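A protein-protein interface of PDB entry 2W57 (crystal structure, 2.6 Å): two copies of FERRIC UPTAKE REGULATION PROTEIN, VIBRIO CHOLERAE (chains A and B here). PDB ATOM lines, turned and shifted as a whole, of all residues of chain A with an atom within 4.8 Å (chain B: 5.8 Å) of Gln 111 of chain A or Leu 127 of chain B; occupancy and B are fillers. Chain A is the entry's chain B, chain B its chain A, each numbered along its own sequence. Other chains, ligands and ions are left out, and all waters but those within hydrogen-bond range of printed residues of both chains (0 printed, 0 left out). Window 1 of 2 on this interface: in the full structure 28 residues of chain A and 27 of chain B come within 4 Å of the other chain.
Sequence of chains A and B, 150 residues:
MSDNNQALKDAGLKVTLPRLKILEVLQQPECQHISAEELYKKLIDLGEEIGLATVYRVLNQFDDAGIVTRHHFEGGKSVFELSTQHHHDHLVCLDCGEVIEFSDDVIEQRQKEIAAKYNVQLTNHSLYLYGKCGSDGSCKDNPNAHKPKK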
ATOM      1  N   ILE A 107       3.617  18.712  14.490  1.00  0.00           N
ATOM      2  CA  ILE A 107       3.183  17.324  14.667  1.00  0.00           C
ATOM      3  C   ILE A 107       4.379  16.372  14.721  1.00  0.00           C
ATOM      4  O   ILE A 107       4.482  15.566  15.658  1.00  0.00           O
ATOM      5  CB  ILE A 107       2.241  16.851  13.545  1.00  0.00           C
ATOM      6  CG1 ILE A 107       0.820  17.366  13.763  1.00  0.00           C
ATOM      7  CG2 ILE A 107       2.190  15.337  13.491  1.00  0.00           C
ATOM      8  CD1 ILE A 107      -0.070  17.209  12.546  1.00  0.00           C
ATOM      9  N   GLU A 108       5.273  16.475  13.724  1.00  0.00           N
ATOM     10  CA  GLU A 108       6.480  15.642  13.650  1.00  0.00           C
ATOM     11  C   GLU A 108       7.371  15.762  14.893  1.00  0.00           C
ATOM     12  O   GLU A 108       7.964  14.779  15.338  1.00  0.00           O
ATOM     13  CB  GLU A 108       7.296  15.945  12.382  1.00  0.00           C
ATOM     14  CG  GLU A 108       6.539  15.825  11.061  1.00  0.00           C
ATOM     15  CD  GLU A 108       5.950  14.431  10.818  1.00  0.00           C
ATOM     16  OE1 GLU A 108       6.634  13.424  11.132  1.00  0.00           O
ATOM     17  OE2 GLU A 108       4.801  14.347  10.306  1.00  0.00           O
ATOM     18  N   GLN A 109       7.458  16.974  15.440  1.00  0.00           N
ATOM     19  CA  GLN A 109       8.210  17.249  16.677  1.00  0.00           C
ATOM     20  C   GLN A 109       7.517  16.665  17.932  1.00  0.00           C
ATOM     21  O   GLN A 109       8.162  16.042  18.795  1.00  0.00           O
ATOM     22  CB  GLN A 109       8.426  18.768  16.810  1.00  0.00           C
ATOM     23  CG  GLN A 109       8.961  19.268  18.160  1.00  0.00           C
ATOM     24  CD  GLN A 109      10.272  18.614  18.539  1.00  0.00           C
ATOM     25  OE1 GLN A 109      11.111  18.319  17.677  1.00  0.00           O
ATOM     26  NE2 GLN A 109      10.457  18.374  19.832  1.00  0.00           N
ATOM     27  N   ARG A 110       6.204  16.867  18.023  1.00  0.00           N
ATOM     28  CA  ARG A 110       5.429  16.355  19.148  1.00  0.00           C
ATOM     29  C   ARG A 110       5.494  14.835  19.211  1.00  0.00           C
ATOM     30  O   ARG A 110       5.589  14.259  20.298  1.00  0.00           O
ATOM     31  CB  ARG A 110       3.967  16.807  19.054  1.00  0.00           C
ATOM     32  CG  ARG A 110       3.702  18.238  19.498  1.00  0.00           C
ATOM     33  CD  ARG A 110       4.138  18.495  20.942  1.00  0.00           C
ATOM     34  NE  ARG A 110       3.728  17.423  21.854  1.00  0.00           N
ATOM     35  CZ  ARG A 110       4.094  17.325  23.131  1.00  0.00           C
ATOM     36  NH1 ARG A 110       4.875  18.251  23.683  1.00  0.00           N
ATOM     37  NH2 ARG A 110       3.666  16.300  23.860  1.00  0.00           N
ATOM     38  N   GLN A 111       5.447  14.202  18.040  1.00  0.00           N
ATOM     39  CA  GLN A 111       5.521  12.744  17.927  1.00  0.00           C
ATOM     40  C   GLN A 111       6.823  12.216  18.513  1.00  0.00           C
ATOM     41  O   GLN A 111       6.824  11.227  19.247  1.00  0.00           O
ATOM     42  CB  GLN A 111       5.361  12.294  16.463  1.00  0.00           C
ATOM     43  CG  GLN A 111       3.943  12.471  15.901  1.00  0.00           C
ATOM     44  CD  GLN A 111       3.806  12.101  14.436  1.00  0.00           C
ATOM     45  OE1 GLN A 111       4.791  11.793  13.763  1.00  0.00           O
ATOM     46  NE2 GLN A 111       2.577  12.132  13.931  1.00  0.00           N
ATOM     47  N   LYS A 112       7.926  12.894  18.198  1.00  0.00           N
ATOM     48  CA  LYS A 112       9.250  12.517  18.698  1.00  0.00           C
ATOM     49  C   LYS A 112       9.306  12.619  20.217  1.00  0.00           C
ATOM     50  O   LYS A 112       9.856  11.736  20.874  1.00  0.00           O
ATOM     51  CB  LYS A 112      10.347  13.373  18.057  1.00  0.00           C
ATOM     52  CG  LYS A 112      10.691  12.967  16.638  1.00  0.00           C
ATOM     53  CD  LYS A 112      11.698  13.921  15.986  1.00  0.00           C
ATOM     54  CE  LYS A 112      12.045  13.484  14.549  1.00  0.00           C
ATOM     55  NZ  LYS A 112      12.860  14.507  13.814  1.00  0.00           N
ATOM     56  N   GLU A 113       8.710  13.680  20.762  1.00  0.00           N
ATOM     57  CA  GLU A 113       8.684  13.918  22.213  1.00  0.00           C
ATOM     58  C   GLU A 113       7.873  12.862  22.962  1.00  0.00           C
ATOM     59  O   GLU A 113       8.258  12.432  24.051  1.00  0.00           O
ATOM     60  CB  GLU A 113       8.142  15.319  22.524  1.00  0.00           C
ATOM     61  CG  GLU A 113       9.052  16.458  22.076  1.00  0.00           C
ATOM     62  CD  GLU A 113       8.402  17.836  22.219  1.00  0.00           C
ATOM     63  OE1 GLU A 113       7.161  17.913  22.405  1.00  0.00           O
ATOM     64  OE2 GLU A 113       9.132  18.849  22.147  1.00  0.00           O
ATOM     65  N   ILE A 114       6.757  12.449  22.365  1.00  0.00           N
ATOM     66  CA  ILE A 114       5.852  11.456  22.955  1.00  0.00           C
ATOM     67  C   ILE A 114       6.496  10.070  23.080  1.00  0.00           C
ATOM     68  O   ILE A 114       6.393   9.424  24.121  1.00  0.00           O
ATOM     69  CB  ILE A 114       4.547  11.368  22.144  1.00  0.00           C
ATOM     70  CG1 ILE A 114       3.726  12.637  22.348  1.00  0.00           C
ATOM     71  CG2 ILE A 114       3.732  10.152  22.542  1.00  0.00           C
ATOM     72  CD1 ILE A 114       2.611  12.800  21.348  1.00  0.00           C
ATOM     73  N   ALA A 115       7.159   9.636  22.007  1.00  0.00           N
ATOM     74  CA  ALA A 115       7.865   8.349  21.961  1.00  0.00           C
ATOM     75  C   ALA A 115       9.065   8.319  22.909  1.00  0.00           C
ATOM     76  O   ALA A 115       9.322   7.308  23.573  1.00  0.00           O
ATOM     77  CB  ALA A 115       8.316   8.040  20.530  1.00  0.00           C
ATOM     78  N   LEU A 122      11.222   5.727  17.488  1.00  0.00           N
ATOM     79  CA  LEU A 122      10.315   5.675  16.346  1.00  0.00           C
ATOM     80  C   LEU A 122      11.009   5.056  15.154  1.00  0.00           C
ATOM     81  O   LEU A 122      12.141   5.417  14.857  1.00  0.00           O
ATOM     82  CB  LEU A 122       9.857   7.076  15.973  1.00  0.00           C
ATOM     83  CG  LEU A 122       8.865   7.713  16.923  1.00  0.00           C
ATOM     84  CD1 LEU A 122       8.721   9.175  16.573  1.00  0.00           C
ATOM     85  CD2 LEU A 122       7.513   6.979  16.863  1.00  0.00           C
ATOM     86  N   HIS A 125       5.563   5.794  11.105  1.00  0.00           N
ATOM     87  CA  HIS A 125       4.280   6.267  11.580  1.00  0.00           C
ATOM     88  C   HIS A 125       3.338   6.529  10.422  1.00  0.00           C
ATOM     89  O   HIS A 125       3.769   6.849   9.309  1.00  0.00           O
ATOM     90  CB  HIS A 125       4.436   7.539  12.437  1.00  0.00           C
ATOM     91  CG  HIS A 125       4.907   8.751  11.684  1.00  0.00           C
ATOM     92  ND1 HIS A 125       6.245   9.068  11.533  1.00  0.00           N
ATOM     93  CD2 HIS A 125       4.218   9.752  11.085  1.00  0.00           C
ATOM     94  CE1 HIS A 125       6.358  10.195  10.851  1.00  0.00           C
ATOM     95  NE2 HIS A 125       5.143  10.631  10.566  1.00  0.00           N
ATOM     96  N   SER A 126       2.044   6.388  10.684  1.00  0.00           N
ATOM     97  CA  SER A 126       1.050   6.827   9.721  1.00  0.00           C
ATOM     98  C   SER A 126       0.102   7.823  10.361  1.00  0.00           C
ATOM     99  O   SER A 126      -0.254   7.693  11.538  1.00  0.00           O
ATOM    100  CB  SER A 126       0.286   5.644   9.123  1.00  0.00           C
ATOM    101  OG  SER A 126      -0.061   4.737  10.133  1.00  0.00           O
ATOM    102  N   LEU A 127      -0.288   8.826   9.580  1.00  0.00           N
ATOM    103  CA  LEU A 127      -1.251   9.831  10.020  1.00  0.00           C
ATOM    104  C   LEU A 127      -2.264  10.090   8.914  1.00  0.00           C
ATOM    105  O   LEU A 127      -1.946  10.702   7.888  1.00  0.00           O
ATOM    106  CB  LEU A 127      -0.536  11.122  10.425  1.00  0.00           C
ATOM    107  CG  LEU A 127      -1.283  12.438  10.697  1.00  0.00           C
ATOM    108  CD1 LEU A 127      -2.391  12.287  11.733  1.00  0.00           C
ATOM    109  CD2 LEU A 127      -0.277  13.516  11.137  1.00  0.00           C
ATOM    110  N   ASP B  89      -4.886   7.747  20.538  1.00  0.00           N
ATOM    111  CA  ASP B  89      -4.064   7.315  19.424  1.00  0.00           C
ATOM    112  C   ASP B  89      -3.093   6.283  19.951  1.00  0.00           C
ATOM    113  O   ASP B  89      -3.121   5.974  21.142  1.00  0.00           O
ATOM    114  CB  ASP B  89      -3.354   8.509  18.806  1.00  0.00           C
ATOM    115  CG  ASP B  89      -4.327   9.505  18.258  1.00  0.00           C
ATOM    116  OD1 ASP B  89      -5.193   9.087  17.457  1.00  0.00           O
ATOM    117  OD2 ASP B  89      -4.256  10.689  18.645  1.00  0.00           O
ATOM    118  N   HIS B  90      -2.252   5.733  19.082  1.00  0.00           N
ATOM    119  CA  HIS B  90      -1.507   4.544  19.463  1.00  0.00           C
ATOM    120  C   HIS B  90      -0.042   4.619  19.144  1.00  0.00           C
ATOM    121  O   HIS B  90       0.362   5.038  18.070  1.00  0.00           O
ATOM    122  CB  HIS B  90      -2.122   3.285  18.839  1.00  0.00           C
ATOM    123  CG  HIS B  90      -3.605   3.177  19.028  1.00  0.00           C
ATOM    124  ND1 HIS B  90      -4.507   3.871  18.245  1.00  0.00           N
ATOM    125  CD2 HIS B  90      -4.344   2.459  19.907  1.00  0.00           C
ATOM    126  CE1 HIS B  90      -5.737   3.588  18.640  1.00  0.00           C
ATOM    127  NE2 HIS B  90      -5.666   2.729  19.642  1.00  0.00           N
ATOM    128  N   LEU B  91       0.746   4.209  20.117  1.00  0.00           N
ATOM    129  CA  LEU B  91       2.169   4.061  19.955  1.00  0.00           C
ATOM    130  C   LEU B  91       2.409   2.567  20.079  1.00  0.00           C
ATOM    131  O   LEU B  91       1.955   1.939  21.026  1.00  0.00           O
ATOM    132  CB  LEU B  91       2.883   4.864  21.044  1.00  0.00           C
ATOM    133  CG  LEU B  91       4.391   4.805  21.272  1.00  0.00           C
ATOM    134  CD1 LEU B  91       5.149   5.447  20.134  1.00  0.00           C
ATOM    135  CD2 LEU B  91       4.710   5.499  22.595  1.00  0.00           C
ATOM    136  N   PHE B 102      -2.196   7.320  23.778  1.00  0.00           N
ATOM    137  CA  PHE B 102      -1.914   8.709  24.126  1.00  0.00           C
ATOM    138  C   PHE B 102      -2.927   9.635  23.474  1.00  0.00           C
ATOM    139  O   PHE B 102      -3.616   9.250  22.529  1.00  0.00           O
ATOM    140  CB  PHE B 102      -0.477   9.105  23.744  1.00  0.00           C
ATOM    141  CG  PHE B 102      -0.238   9.202  22.255  1.00  0.00           C
ATOM    142  CD1 PHE B 102       0.102   8.071  21.512  1.00  0.00           C
ATOM    143  CD2 PHE B 102      -0.346  10.426  21.598  1.00  0.00           C
ATOM    144  CE1 PHE B 102       0.325   8.155  20.137  1.00  0.00           C
ATOM    145  CE2 PHE B 102      -0.124  10.518  20.225  1.00  0.00           C
ATOM    146  CZ  PHE B 102       0.211   9.375  19.494  1.00  0.00           C
ATOM    147  N   ILE B 107      -0.891  17.992  18.986  1.00  0.00           N
ATOM    148  CA  ILE B 107      -1.207  17.205  17.802  1.00  0.00           C
ATOM    149  C   ILE B 107      -2.687  17.331  17.451  1.00  0.00           C
ATOM    150  O   ILE B 107      -3.021  17.657  16.311  1.00  0.00           O
ATOM    151  CB  ILE B 107      -0.800  15.723  17.955  1.00  0.00           C
ATOM    152  CG1 ILE B 107       0.724  15.607  18.041  1.00  0.00           C
ATOM    153  CG2 ILE B 107      -1.354  14.881  16.790  1.00  0.00           C
ATOM    154  CD1 ILE B 107       1.210  14.262  18.479  1.00  0.00           C
ATOM    155  N   GLN B 111      -3.832  19.083  13.670  1.00  0.00           N
ATOM    156  CA  GLN B 111      -4.675  18.376  12.698  1.00  0.00           C
ATOM    157  C   GLN B 111      -5.820  19.254  12.171  1.00  0.00           C
ATOM    158  O   GLN B 111      -6.049  19.317  10.959  1.00  0.00           O
ATOM    159  CB  GLN B 111      -5.218  17.073  13.317  1.00  0.00           C
ATOM    160  CG  GLN B 111      -4.128  16.068  13.740  1.00  0.00           C
ATOM    161  CD  GLN B 111      -4.667  14.810  14.409  1.00  0.00           C
ATOM    162  OE1 GLN B 111      -5.843  14.731  14.760  1.00  0.00           O
ATOM    163  NE2 GLN B 111      -3.797  13.825  14.605  1.00  0.00           N
ATOM    164  N   HIS B 125      -9.804  11.071  12.316  1.00  0.00           N
ATOM    165  CA  HIS B 125      -8.406  10.808  11.985  1.00  0.00           C
ATOM    166  C   HIS B 125      -7.944   9.478  12.585  1.00  0.00           C
ATOM    167  O   HIS B 125      -8.646   8.875  13.389  1.00  0.00           O
ATOM    168  CB  HIS B 125      -7.514  11.963  12.449  1.00  0.00           C
ATOM    169  CG  HIS B 125      -7.350  12.057  13.937  1.00  0.00           C
ATOM    170  ND1 HIS B 125      -8.263  12.698  14.749  1.00  0.00           N
ATOM    171  CD2 HIS B 125      -6.369  11.613  14.756  1.00  0.00           C
ATOM    172  CE1 HIS B 125      -7.857  12.637  16.004  1.00  0.00           C
ATOM    173  NE2 HIS B 125      -6.708  11.987  16.036  1.00  0.00           N
ATOM    174  N   SER B 126      -6.777   9.002  12.175  1.00  0.00           N
ATOM    175  CA  SER B 126      -6.138   7.899  12.887  1.00  0.00           C
ATOM    176  C   SER B 126      -4.638   8.094  12.863  1.00  0.00           C
ATOM    177  O   SER B 126      -4.080   8.475  11.835  1.00  0.00           O
ATOM    178  CB  SER B 126      -6.537   6.530  12.304  1.00  0.00           C
ATOM    179  OG  SER B 126      -6.168   6.408  10.941  1.00  0.00           O
ATOM    180  N   LEU B 127      -3.997   7.853  14.003  1.00  0.00           N
ATOM    181  CA  LEU B 127      -2.551   8.070  14.138  1.00  0.00           C
ATOM    182  C   LEU B 127      -1.885   6.892  14.833  1.00  0.00           C
ATOM    183  O   LEU B 127      -2.292   6.511  15.931  1.00  0.00           O
ATOM    184  CB  LEU B 127      -2.259   9.390  14.872  1.00  0.00           C
ATOM    185  CG  LEU B 127      -0.868   9.714  15.417  1.00  0.00           C
ATOM    186  CD1 LEU B 127       0.148   9.877  14.308  1.00  0.00           C
ATOM    187  CD2 LEU B 127      -0.916  10.967  16.275  1.00  0.00           C
ATOM    188  N   TYR B 128      -0.873   6.325  14.169  1.00  0.00           N
ATOM    189  CA  TYR B 128      -0.135   5.167  14.668  1.00  0.00           C
ATOM    190  C   TYR B 128       1.354   5.448  14.630  1.00  0.00           C
ATOM    191  O   TYR B 128       1.914   5.722  13.571  1.00  0.00           O
ATOM    192  CB  TYR B 128      -0.443   3.910  13.837  1.00  0.00           C
ATOM    193  CG  TYR B 128      -1.891   3.510  13.871  1.00  0.00           C
ATOM    194  CD1 TYR B 128      -2.422   2.849  14.971  1.00  0.00           C
ATOM    195  CD2 TYR B 128      -2.741   3.823  12.819  1.00  0.00           C
ATOM    196  CE1 TYR B 128      -3.774   2.506  15.018  1.00  0.00           C
ATOM    197  CE2 TYR B 128      -4.089   3.485  12.853  1.00  0.00           C
ATOM    198  CZ  TYR B 128      -4.599   2.830  13.951  1.00  0.00           C
ATOM    199  OH  TYR B 128      -5.936   2.488  13.986  1.00  0.00           O
ATOM    200  N   LEU B 129       1.993   5.393  15.790  1.00  0.00           N
ATOM    201  CA  LEU B 129       3.434   5.554  15.863  1.00  0.00           C
ATOM    202  C   LEU B 129       4.040   4.184  16.106  1.00  0.00           C
ATOM    203  O   LEU B 129       3.597   3.462  17.001  1.00  0.00           O
ATOM    204  CB  LEU B 129       3.806   6.525  16.990  1.00  0.00           C
ATOM    205  CG  LEU B 129       3.095   7.881  16.996  1.00  0.00           C
ATOM    206  CD1 LEU B 129       3.515   8.737  18.190  1.00  0.00           C
ATOM    207  CD2 LEU B 129       3.321   8.638  15.692  1.00  0.00           C
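Arg 110 of chain A touches Ile 107 of chain B.
Leu 127 of chain B touches Gln 111 of chain A.
Gln 111 of chain A touches Leu 129 of chain B (CD to CD2, 3.7 Å).
Ile 114 of chain A touches Phe 102 of chain B (CD1 to CE2, 3.7 Å).
Ile 107 of chain B touches Ile 114 of chain A (CD1 to CD1, 3.5 Å).
Tyr 128 of chain B touches His 125 of chain A (O to CA, 3.1 Å).
His 125 of chain A touches Leu 129 of chain B (CB to CD2, 3.6 Å).
Ser 126 of chain A touches Leu 127 of chain B.
Leu 127 of chain A touches Gln 111 of chain B.
Ser 126 of chain B touches Leu 127 of chain A (O to CA, 3.6 Å).
A ring nitrogen (NE2) of His 125 of chain A sits close to the side-chain amide oxygen (OE1) of Gln 111 of chain A (3.4 Å).
N of His 90 of chain B is in hydrogen-bond range of O of Leu 127 of chain B, at 3.2 Å.
The backbone NH (N) of Leu 129 of chain B is in hydrogen-bond range of the backbone carbonyl oxygen (O) of His 90 of chain B, 2.8 Å away.
The guanidinium group (NH1) of Arg 110 of chain A lies within salt-bridge range of the side-chain carboxylate (OE1) of Glu 113 of chain A.
OE1 of Gln 111 of chain B sits close to ND1 of His 125 of chain B (3.2 Å).
O of Phe 102 of chain B lies within hydrogen-bond range of N of Asp 89 of chain B.
The backbone carbonyl oxygen (O) of Tyr 128 of chain B lies within hydrogen-bond range of the backbone NH (N) of Ser 126 of chain A (3.0 Å).
Of chain B, only Leu 127 and Leu 129 come within 4 Å of Gln 111 of chain A.
Of chain A, only Gln 111 (3.3 Å) and Ser 126 (3.5 Å) come within 4 Å of Leu 127 of chain B.
Of the printed residues of chain A, Phe 102 of chain B touches Ile 114 (3.7 Å).
Printed residues of chain B within 4 Å of Arg 110 of chain A: Ile 107 (3.6 Å).
Of the printed residues of chain B, Ser 126 of chain A touches Ser 126, Leu 127 and Tyr 128.
Glu 113 of chain A touches none of the printed residues of chain B.
The nearest residue of chain A that does not touch Leu 127 of chain B is Leu 127 of chain A (4.1 Å).
Hydrophobic or aromatic side chains of chain B that line the printed part of chain A: Phe 102, Ile 107, Leu 127, Tyr 128 and Leu 129.
Hydrophobic or aromatic side chains of chain A that line the printed part of chain B: Ile 114, Leu 122, His 125 and Leu 127.
Gln 111 of chain A touches Leu 127 of chain B, and with the chains exchanged Leu 127 of chain A touches Gln 111 of chain B.
Ser 126 of chain A touches its own counterpart, Ser 126 of chain B.
Ser 126 of chain A touches Leu 127 of chain B, and with the chains exchanged Leu 127 of chain A touches Ser 126 of chain B.
5 positions are printed for both chains.
Of the 13 pairs that touch across the chains among the printed residues, 5 have their exchanged pair printed and touching as well.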
